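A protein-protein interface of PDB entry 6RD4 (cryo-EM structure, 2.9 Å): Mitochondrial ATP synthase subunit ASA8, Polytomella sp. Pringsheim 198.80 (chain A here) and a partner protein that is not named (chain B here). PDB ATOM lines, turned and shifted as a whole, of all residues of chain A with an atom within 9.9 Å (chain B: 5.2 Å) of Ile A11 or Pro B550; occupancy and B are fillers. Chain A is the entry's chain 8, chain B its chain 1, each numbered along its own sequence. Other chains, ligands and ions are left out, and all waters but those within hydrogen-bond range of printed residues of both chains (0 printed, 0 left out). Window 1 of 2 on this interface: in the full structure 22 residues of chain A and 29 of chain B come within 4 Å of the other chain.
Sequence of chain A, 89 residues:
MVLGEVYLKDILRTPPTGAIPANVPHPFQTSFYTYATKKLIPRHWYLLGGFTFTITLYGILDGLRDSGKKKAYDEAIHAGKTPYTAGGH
O of His B547 lies within hydrogen-bond range of NH2 of Arg A13, at 3.0 Å. N of Arg A13 is in hydrogen-bond range of O of Met B548, 3.0 Å away.
The side-chain amino group (NZ) of Lys A9 lies within salt-bridge range of the side-chain carboxylate (OD2) of Asp A10 (2.7 Å). The guanidinium group of Arg A13 lies within salt-bridge range of the side-chain carboxylate of Asp A10.
Among the printed residues, pairs that only touch across the chains: Leu A3 with Pro B594, Tyr A7 with Pro B594, Tyr A7 with Arg B597, Leu A8 with Pro B594, Asp A10 with Leu B551, Ile A11 with Pro B550, Ile A11 with His B590, Ile A11 with Leu B593, Ile A11 with Pro B594, Leu A12 with Met B548, Arg A13 with Pro B550, Thr A14 with His B547, Thr A14 with Met B548 and Val A24 with Ala B546.
Of the printed residues of chain B, Asp A10 touches Leu B551. Printed residues of chain B within 4 Å of Ile A11: Pro B550, His B590, Leu B593 and Pro B594. Printed residues of chain B within 4 Å of Arg A13: His B547 (3.0 Å), Met B548 (3.0 Å) and Pro B550 (3.6 Å). Ala B546 touches just one residue of chain A: Val A24. Pro B550 touches just these residues of chain A: Ile A11 (3.6 Å) and Arg A13 (3.6 Å). Of the printed residues of chain A, Leu B551 touches Asp A10 (3.98 Å). Printed residues of chain A within 4 Å of His B590: Ile A11. Leu B593 touches just one residue of chain A: Ile A11 (3.8 Å). Printed residues of chain A within 4 Å of Pro B594: Leu A3, Tyr A7, Leu A8 and Ile A11. The nearest printed residue of chain B that does not touch Ile A11 is Asp B549 (4.02 Å).
Hydrophobic or aromatic side chains of chain A that line the printed part of chain B: Leu A3, Tyr A7, Leu A8, Ile A11 and Val A24. Of the 14 printed residues of chain B, 9 touch a printed residue of chain A. Hydrophobic or aromatic side chains of chain B within 4 Å of the printed part of chain A: Ala B546, His B547, Met B548, Pro B550, Leu B551, Leu B593 and Pro B594. Among the printed residues, 16 pairs touch across the chains. Among the printed residues, no Asp or Glu carboxylate lies within 4 Å of a Lys or Arg side-chain nitrogen of the other chain.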
ATOM      1  N   LEU A   3      -2.169 -33.936  -6.652  1.00  0.00           N
ATOM      2  CA  LEU A   3      -1.870 -32.516  -6.698  1.00  0.00           C
ATOM      3  C   LEU A   3      -0.774 -32.328  -7.726  1.00  0.00           C
ATOM      4  O   LEU A   3       0.338 -32.827  -7.550  1.00  0.00           O
ATOM      5  CB  LEU A   3      -1.441 -32.016  -5.330  1.00  0.00           C
ATOM      6  CG  LEU A   3      -1.686 -30.566  -4.986  1.00  0.00           C
ATOM      7  CD1 LEU A   3      -1.892 -30.498  -3.530  1.00  0.00           C
ATOM      8  CD2 LEU A   3      -0.525 -29.721  -5.377  1.00  0.00           C
ATOM      9  N   GLU A   5       0.796 -29.637  -9.974  1.00  0.00           N
ATOM     10  CA  GLU A   5       1.621 -28.538 -10.482  1.00  0.00           C
ATOM     11  C   GLU A   5       0.838 -27.471 -11.226  1.00  0.00           C
ATOM     12  O   GLU A   5       1.370 -26.400 -11.513  1.00  0.00           O
ATOM     13  CB  GLU A   5       2.750 -29.043 -11.382  1.00  0.00           C
ATOM     14  CG  GLU A   5       3.989 -28.214 -11.328  1.00  0.00           C
ATOM     15  CD  GLU A   5       4.796 -28.334 -12.589  1.00  0.00           C
ATOM     16  OE1 GLU A   5       4.703 -29.384 -13.250  1.00  0.00           O
ATOM     17  OE2 GLU A   5       5.511 -27.372 -12.935  1.00  0.00           O
ATOM     18  N   VAL A   6      -0.428 -27.704 -11.515  1.00  0.00           N
ATOM     19  CA  VAL A   6      -1.265 -26.601 -11.931  1.00  0.00           C
ATOM     20  C   VAL A   6      -1.802 -25.896 -10.700  1.00  0.00           C
ATOM     21  O   VAL A   6      -2.242 -24.745 -10.791  1.00  0.00           O
ATOM     22  CB  VAL A   6      -2.377 -27.101 -12.869  1.00  0.00           C
ATOM     23  CG1 VAL A   6      -3.466 -27.788 -12.105  1.00  0.00           C
ATOM     24  CG2 VAL A   6      -2.919 -25.985 -13.724  1.00  0.00           C
ATOM     25  N   TYR A   7      -1.730 -26.533  -9.540  1.00  0.00           N
ATOM     26  CA  TYR A   7      -2.149 -25.910  -8.306  1.00  0.00           C
ATOM     27  C   TYR A   7      -1.036 -25.128  -7.656  1.00  0.00           C
ATOM     28  O   TYR A   7      -1.315 -24.198  -6.904  1.00  0.00           O
ATOM     29  CB  TYR A   7      -2.668 -26.960  -7.333  1.00  0.00           C
ATOM     30  CG  TYR A   7      -3.896 -27.652  -7.818  1.00  0.00           C
ATOM     31  CD1 TYR A   7      -5.117 -27.016  -7.786  1.00  0.00           C
ATOM     32  CD2 TYR A   7      -3.842 -28.936  -8.302  1.00  0.00           C
ATOM     33  CE1 TYR A   7      -6.242 -27.635  -8.224  1.00  0.00           C
ATOM     34  CE2 TYR A   7      -4.960 -29.564  -8.748  1.00  0.00           C
ATOM     35  CZ  TYR A   7      -6.158 -28.910  -8.707  1.00  0.00           C
ATOM     36  OH  TYR A   7      -7.285 -29.543  -9.155  1.00  0.00           O
ATOM     37  N   LEU A   8       0.204 -25.475  -7.933  1.00  0.00           N
ATOM     38  CA  LEU A   8       1.347 -24.745  -7.427  1.00  0.00           C
ATOM     39  C   LEU A   8       1.810 -23.651  -8.361  1.00  0.00           C
ATOM     40  O   LEU A   8       2.856 -23.064  -8.112  1.00  0.00           O
ATOM     41  CB  LEU A   8       2.520 -25.682  -7.205  1.00  0.00           C
ATOM     42  CG  LEU A   8       2.511 -26.868  -6.280  1.00  0.00           C
ATOM     43  CD1 LEU A   8       3.758 -27.518  -6.593  1.00  0.00           C
ATOM     44  CD2 LEU A   8       2.587 -26.433  -4.898  1.00  0.00           C
ATOM     45  N   LYS A   9       1.102 -23.388  -9.447  1.00  0.00           N
ATOM     46  CA  LYS A   9       1.588 -22.437 -10.431  1.00  0.00           C
ATOM     47  C   LYS A   9       1.427 -21.020  -9.926  1.00  0.00           C
ATOM     48  O   LYS A   9       0.337 -20.625  -9.512  1.00  0.00           O
ATOM     49  CB  LYS A   9       0.844 -22.596 -11.745  1.00  0.00           C
ATOM     50  CG  LYS A   9       1.479 -21.848 -12.876  1.00  0.00           C
ATOM     51  CD  LYS A   9       0.593 -21.828 -14.078  1.00  0.00           C
ATOM     52  CE  LYS A   9      -0.511 -20.809 -13.930  1.00  0.00           C
ATOM     53  NZ  LYS A   9      -0.057 -19.443 -14.269  1.00  0.00           N
ATOM     54  N   ASP A  10       2.536 -20.276  -9.952  1.00  0.00           N
ATOM     55  CA  ASP A  10       2.643 -18.882  -9.529  1.00  0.00           C
ATOM     56  C   ASP A  10       2.309 -18.701  -8.062  1.00  0.00           C
ATOM     57  O   ASP A  10       1.877 -17.634  -7.647  1.00  0.00           O
ATOM     58  CB  ASP A  10       1.789 -17.961 -10.391  1.00  0.00           C
ATOM     59  CG  ASP A  10       2.193 -17.989 -11.836  1.00  0.00           C
ATOM     60  OD1 ASP A  10       3.370 -18.279 -12.116  1.00  0.00           O
ATOM     61  OD2 ASP A  10       1.343 -17.709 -12.699  1.00  0.00           O
ATOM     62  N   ILE A  11       2.511 -19.739  -7.270  1.00  0.00           N
ATOM     63  CA  ILE A  11       2.241 -19.712  -5.848  1.00  0.00           C
ATOM     64  C   ILE A  11       3.511 -20.142  -5.149  1.00  0.00           C
ATOM     65  O   ILE A  11       4.047 -19.420  -4.306  1.00  0.00           O
ATOM     66  CB  ILE A  11       1.069 -20.622  -5.473  1.00  0.00           C
ATOM     67  CG1 ILE A  11      -0.233 -20.049  -5.992  1.00  0.00           C
ATOM     68  CG2 ILE A  11       0.966 -20.716  -4.020  1.00  0.00           C
ATOM     69  CD1 ILE A  11      -1.383 -20.950  -5.848  1.00  0.00           C
ATOM     70  N   LEU A  12       4.005 -21.318  -5.504  1.00  0.00           N
ATOM     71  CA  LEU A  12       5.189 -21.897  -4.900  1.00  0.00           C
ATOM     72  C   LEU A  12       6.069 -22.424  -6.001  1.00  0.00           C
ATOM     73  O   LEU A  12       5.648 -23.293  -6.759  1.00  0.00           O
ATOM     74  CB  LEU A  12       4.836 -23.038  -3.961  1.00  0.00           C
ATOM     75  CG  LEU A  12       4.206 -22.748  -2.621  1.00  0.00           C
ATOM     76  CD1 LEU A  12       3.597 -24.013  -2.195  1.00  0.00           C
ATOM     77  CD2 LEU A  12       5.254 -22.343  -1.664  1.00  0.00           C
ATOM     78  N   ARG A  13       7.284 -21.922  -6.089  1.00  0.00           N
ATOM     79  CA  ARG A  13       8.244 -22.444  -7.034  1.00  0.00           C
ATOM     80  C   ARG A  13       9.431 -22.994  -6.272  1.00  0.00           C
ATOM     81  O   ARG A  13       9.660 -22.641  -5.124  1.00  0.00           O
ATOM     82  CB  ARG A  13       8.676 -21.383  -8.003  1.00  0.00           C
ATOM     83  CG  ARG A  13       7.541 -20.621  -8.570  1.00  0.00           C
ATOM     84  CD  ARG A  13       7.951 -19.934  -9.799  1.00  0.00           C
ATOM     85  NE  ARG A  13       6.848 -19.201 -10.376  1.00  0.00           N
ATOM     86  CZ  ARG A  13       6.686 -17.900 -10.267  1.00  0.00           C
ATOM     87  NH1 ARG A  13       5.657 -17.312 -10.832  1.00  0.00           N
ATOM     88  NH2 ARG A  13       7.558 -17.188  -9.606  1.00  0.00           N
ATOM     89  N   THR A  14      10.154 -23.896  -6.903  1.00  0.00           N
ATOM     90  CA  THR A  14      11.341 -24.494  -6.321  1.00  0.00           C
ATOM     91  C   THR A  14      12.540 -23.624  -6.657  1.00  0.00           C
ATOM     92  O   THR A  14      12.401 -22.684  -7.434  1.00  0.00           O
ATOM     93  CB  THR A  14      11.487 -25.903  -6.867  1.00  0.00           C
ATOM     94  OG1 THR A  14      11.365 -25.840  -8.280  1.00  0.00           O
ATOM     95  CG2 THR A  14      10.431 -26.790  -6.288  1.00  0.00           C
ATOM     96  N   ALA A  22      15.633 -12.550 -13.201  1.00  0.00           N
ATOM     97  CA  ALA A  22      15.789 -11.165 -12.828  1.00  0.00           C
ATOM     98  C   ALA A  22      15.084 -10.914 -11.509  1.00  0.00           C
ATOM     99  O   ALA A  22      14.110 -11.584 -11.169  1.00  0.00           O
ATOM    100  CB  ALA A  22      15.224 -10.264 -13.910  1.00  0.00           C
ATOM    101  N   ASN A  23      15.594  -9.950 -10.755  1.00  0.00           N
ATOM    102  CA  ASN A  23      14.944  -9.551  -9.521  1.00  0.00           C
ATOM    103  C   ASN A  23      13.625  -8.876  -9.841  1.00  0.00           C
ATOM    104  O   ASN A  23      13.492  -8.194 -10.855  1.00  0.00           O
ATOM    105  CB  ASN A  23      15.853  -8.622  -8.739  1.00  0.00           C
ATOM    106  CG  ASN A  23      15.453  -8.489  -7.313  1.00  0.00           C
ATOM    107  OD1 ASN A  23      14.479  -9.073  -6.879  1.00  0.00           O
ATOM    108  ND2 ASN A  23      16.221  -7.735  -6.559  1.00  0.00           N
ATOM    109  N   VAL A  24      12.632  -9.119  -9.005  1.00  0.00           N
ATOM    110  CA  VAL A  24      11.325  -8.492  -9.179  1.00  0.00           C
ATOM    111  C   VAL A  24      11.411  -7.054  -8.679  1.00  0.00           C
ATOM    112  O   VAL A  24      11.818  -6.834  -7.534  1.00  0.00           O
ATOM    113  CB  VAL A  24      10.262  -9.271  -8.431  1.00  0.00           C
ATOM    114  CG1 VAL A  24       8.986  -8.533  -8.429  1.00  0.00           C
ATOM    115  CG2 VAL A  24      10.063 -10.558  -9.076  1.00  0.00           C
ATOM    116  N   PRO A  25      11.062  -6.067  -9.486  1.00  0.00           N
ATOM    117  CA  PRO A  25      11.114  -4.692  -9.022  1.00  0.00           C
ATOM    118  C   PRO A  25       9.993  -4.394  -8.056  1.00  0.00           C
ATOM    119  O   PRO A  25       8.890  -4.925  -8.160  1.00  0.00           O
ATOM    120  CB  PRO A  25      10.935  -3.887 -10.306  1.00  0.00           C
ATOM    121  CG  PRO A  25      11.120  -4.821 -11.366  1.00  0.00           C
ATOM    122  CD  PRO A  25      10.659  -6.117 -10.885  1.00  0.00           C
ATOM    123  N   VAL B 545      14.673 -15.575  -4.161  1.00  0.00           N
ATOM    124  CA  VAL B 545      13.588 -15.494  -3.193  1.00  0.00           C
ATOM    125  C   VAL B 545      12.292 -15.121  -3.883  1.00  0.00           C
ATOM    126  O   VAL B 545      11.252 -15.738  -3.664  1.00  0.00           O
ATOM    127  CB  VAL B 545      13.935 -14.473  -2.109  1.00  0.00           C
ATOM    128  CG1 VAL B 545      12.784 -14.254  -1.251  1.00  0.00           C
ATOM    129  CG2 VAL B 545      15.057 -14.932  -1.324  1.00  0.00           C
ATOM    130  N   ALA B 546      12.335 -14.119  -4.742  1.00  0.00           N
ATOM    131  CA  ALA B 546      11.139 -13.695  -5.442  1.00  0.00           C
ATOM    132  C   ALA B 546      10.741 -14.655  -6.528  1.00  0.00           C
ATOM    133  O   ALA B 546       9.637 -14.548  -7.054  1.00  0.00           O
ATOM    134  CB  ALA B 546      11.352 -12.319  -6.036  1.00  0.00           C
ATOM    135  N   HIS B 547      11.630 -15.555  -6.920  1.00  0.00           N
ATOM    136  CA  HIS B 547      11.242 -16.622  -7.815  1.00  0.00           C
ATOM    137  C   HIS B 547      10.540 -17.715  -7.049  1.00  0.00           C
ATOM    138  O   HIS B 547       9.437 -18.116  -7.404  1.00  0.00           O
ATOM    139  CB  HIS B 547      12.460 -17.189  -8.518  1.00  0.00           C
ATOM    140  CG  HIS B 547      12.127 -18.277  -9.474  1.00  0.00           C
ATOM    141  ND1 HIS B 547      12.394 -19.599  -9.222  1.00  0.00           N
ATOM    142  CD2 HIS B 547      11.514 -18.239 -10.675  1.00  0.00           C
ATOM    143  CE1 HIS B 547      11.970 -20.331 -10.231  1.00  0.00           C
ATOM    144  NE2 HIS B 547      11.426 -19.530 -11.125  1.00  0.00           N
ATOM    145  N   MET B 548      11.169 -18.180  -5.979  1.00  0.00           N
ATOM    146  CA  MET B 548      10.636 -19.262  -5.178  1.00  0.00           C
ATOM    147  C   MET B 548       9.354 -18.862  -4.487  1.00  0.00           C
ATOM    148  O   MET B 548       8.381 -19.613  -4.492  1.00  0.00           O
ATOM    149  CB  MET B 548      11.660 -19.678  -4.147  1.00  0.00           C
ATOM    150  CG  MET B 548      12.640 -20.637  -4.602  1.00  0.00           C
ATOM    151  SD  MET B 548      13.341 -21.336  -3.149  1.00  0.00           S
ATOM    152  CE  MET B 548      14.580 -20.147  -2.853  1.00  0.00           C
ATOM    153  N   ASP B 549       9.318 -17.686  -3.889  1.00  0.00           N
ATOM    154  CA  ASP B 549       8.153 -17.235  -3.144  1.00  0.00           C
ATOM    155  C   ASP B 549       7.691 -15.913  -3.723  1.00  0.00           C
ATOM    156  O   ASP B 549       8.056 -14.851  -3.219  1.00  0.00           O
ATOM    157  CB  ASP B 549       8.468 -17.101  -1.666  1.00  0.00           C
ATOM    158  CG  ASP B 549       7.323 -17.525  -0.813  1.00  0.00           C
ATOM    159  OD1 ASP B 549       6.255 -17.780  -1.378  1.00  0.00           O
ATOM    160  OD2 ASP B 549       7.494 -17.674   0.408  1.00  0.00           O
ATOM    161  N   PRO B 550       6.899 -15.938  -4.791  1.00  0.00           N
ATOM    162  CA  PRO B 550       6.518 -14.683  -5.421  1.00  0.00           C
ATOM    163  C   PRO B 550       5.420 -13.954  -4.695  1.00  0.00           C
ATOM    164  O   PRO B 550       5.354 -12.730  -4.792  1.00  0.00           O
ATOM    165  CB  PRO B 550       6.077 -15.129  -6.810  1.00  0.00           C
ATOM    166  CG  PRO B 550       5.645 -16.454  -6.642  1.00  0.00           C
ATOM    167  CD  PRO B 550       6.458 -17.081  -5.591  1.00  0.00           C
ATOM    168  N   LEU B 551       4.546 -14.651  -3.995  1.00  0.00           N
ATOM    169  CA  LEU B 551       3.473 -13.997  -3.281  1.00  0.00           C
ATOM    170  C   LEU B 551       3.872 -13.565  -1.897  1.00  0.00           C
ATOM    171  O   LEU B 551       3.112 -12.860  -1.258  1.00  0.00           O
ATOM    172  CB  LEU B 551       2.265 -14.915  -3.160  1.00  0.00           C
ATOM    173  CG  LEU B 551       1.518 -15.374  -4.389  1.00  0.00           C
ATOM    174  CD1 LEU B 551       0.379 -16.203  -3.959  1.00  0.00           C
ATOM    175  CD2 LEU B 551       1.016 -14.202  -5.112  1.00  0.00           C
ATOM    176  N   LEU B 552       5.006 -14.011  -1.389  1.00  0.00           N
ATOM    177  CA  LEU B 552       5.508 -13.437  -0.154  1.00  0.00           C
ATOM    178  C   LEU B 552       6.143 -12.101  -0.424  1.00  0.00           C
ATOM    179  O   LEU B 552       5.945 -11.150   0.323  1.00  0.00           O
ATOM    180  CB  LEU B 552       6.519 -14.360   0.498  1.00  0.00           C
ATOM    181  CG  LEU B 552       7.131 -13.845   1.781  1.00  0.00           C
ATOM    182  CD1 LEU B 552       6.097 -13.719   2.825  1.00  0.00           C
ATOM    183  CD2 LEU B 552       8.193 -14.731   2.239  1.00  0.00           C
ATOM    184  N   ILE B 553       6.896 -12.013  -1.511  1.00  0.00           N
ATOM    185  CA  ILE B 553       7.472 -10.764  -1.970  1.00  0.00           C
ATOM    186  C   ILE B 553       6.389  -9.792  -2.389  1.00  0.00           C
ATOM    187  O   ILE B 553       6.510  -8.598  -2.154  1.00  0.00           O
ATOM    188  CB  ILE B 553       8.452 -11.098  -3.101  1.00  0.00           C
ATOM    189  CG1 ILE B 553       9.609 -11.908  -2.549  1.00  0.00           C
ATOM    190  CG2 ILE B 553       8.931  -9.913  -3.807  1.00  0.00           C
ATOM    191  CD1 ILE B 553      10.299 -11.290  -1.414  1.00  0.00           C
ATOM    192  N   LYS B 554       5.294 -10.282  -2.955  1.00  0.00           N
ATOM    193  CA  LYS B 554       4.179  -9.435  -3.347  1.00  0.00           C
ATOM    194  C   LYS B 554       3.494  -8.812  -2.148  1.00  0.00           C
ATOM    195  O   LYS B 554       3.093  -7.654  -2.196  1.00  0.00           O
ATOM    196  CB  LYS B 554       3.176 -10.249  -4.143  1.00  0.00           C
ATOM    197  CG  LYS B 554       2.036  -9.472  -4.693  1.00  0.00           C
ATOM    198  CD  LYS B 554       0.858 -10.342  -4.875  1.00  0.00           C
ATOM    199  CE  LYS B 554      -0.283  -9.581  -5.408  1.00  0.00           C
ATOM    200  NZ  LYS B 554      -1.486 -10.420  -5.374  1.00  0.00           N
ATOM    201  N   HIS B 590      -0.578 -18.227   1.775  1.00  0.00           N
ATOM    202  CA  HIS B 590      -0.667 -18.756   0.441  1.00  0.00           C
ATOM    203  C   HIS B 590       0.121 -20.028   0.268  1.00  0.00           C
ATOM    204  O   HIS B 590       0.169 -20.554  -0.836  1.00  0.00           O
ATOM    205  CB  HIS B 590      -0.143 -17.727  -0.531  1.00  0.00           C
ATOM    206  CG  HIS B 590       1.253 -17.301  -0.228  1.00  0.00           C
ATOM    207  ND1 HIS B 590       2.341 -17.849  -0.856  1.00  0.00           N
ATOM    208  CD2 HIS B 590       1.744 -16.415   0.661  1.00  0.00           C
ATOM    209  CE1 HIS B 590       3.440 -17.313  -0.375  1.00  0.00           C
ATOM    210  NE2 HIS B 590       3.104 -16.435   0.544  1.00  0.00           N
ATOM    211  N   LEU B 593      -2.545 -22.566  -0.008  1.00  0.00           N
ATOM    212  CA  LEU B 593      -3.452 -22.402  -1.135  1.00  0.00           C
ATOM    213  C   LEU B 593      -3.359 -23.492  -2.201  1.00  0.00           C
ATOM    214  O   LEU B 593      -4.416 -23.844  -2.746  1.00  0.00           O
ATOM    215  CB  LEU B 593      -3.243 -21.025  -1.762  1.00  0.00           C
ATOM    216  CG  LEU B 593      -4.163 -20.647  -2.902  1.00  0.00           C
ATOM    217  CD1 LEU B 593      -5.556 -20.672  -2.400  1.00  0.00           C
ATOM    218  CD2 LEU B 593      -3.820 -19.317  -3.412  1.00  0.00           C
ATOM    219  N   PRO B 594      -2.201 -24.065  -2.561  1.00  0.00           N
ATOM    220  CA  PRO B 594      -2.247 -25.202  -3.480  1.00  0.00           C
ATOM    221  C   PRO B 594      -2.918 -26.426  -2.920  1.00  0.00           C
ATOM    222  O   PRO B 594      -3.339 -27.281  -3.693  1.00  0.00           O
ATOM    223  CB  PRO B 594      -0.778 -25.473  -3.752  1.00  0.00           C
ATOM    224  CG  PRO B 594      -0.157 -24.253  -3.567  1.00  0.00           C
ATOM    225  CD  PRO B 594      -0.802 -23.637  -2.431  1.00  0.00           C
ATOM    226  N   ARG B 597      -6.976 -25.399  -2.782  1.00  0.00           N
ATOM    227  CA  ARG B 597      -7.569 -25.370  -4.104  1.00  0.00           C
ATOM    228  C   ARG B 597      -7.688 -26.758  -4.677  1.00  0.00           C
ATOM    229  O   ARG B 597      -8.508 -26.983  -5.560  1.00  0.00           O
ATOM    230  CB  ARG B 597      -6.733 -24.538  -5.049  1.00  0.00           C
ATOM    231  CG  ARG B 597      -6.989 -23.112  -4.949  1.00  0.00           C
ATOM    232  CD  ARG B 597      -6.140 -22.374  -5.921  1.00  0.00           C
ATOM    233  NE  ARG B 597      -6.580 -22.512  -7.293  1.00  0.00           N
ATOM    234  CZ  ARG B 597      -7.554 -21.794  -7.825  1.00  0.00           C
ATOM    235  NH1 ARG B 597      -8.198 -20.904  -7.094  1.00  0.00           N
ATOM    236  NH2 ARG B 597      -7.888 -21.960  -9.085  1.00  0.00           N
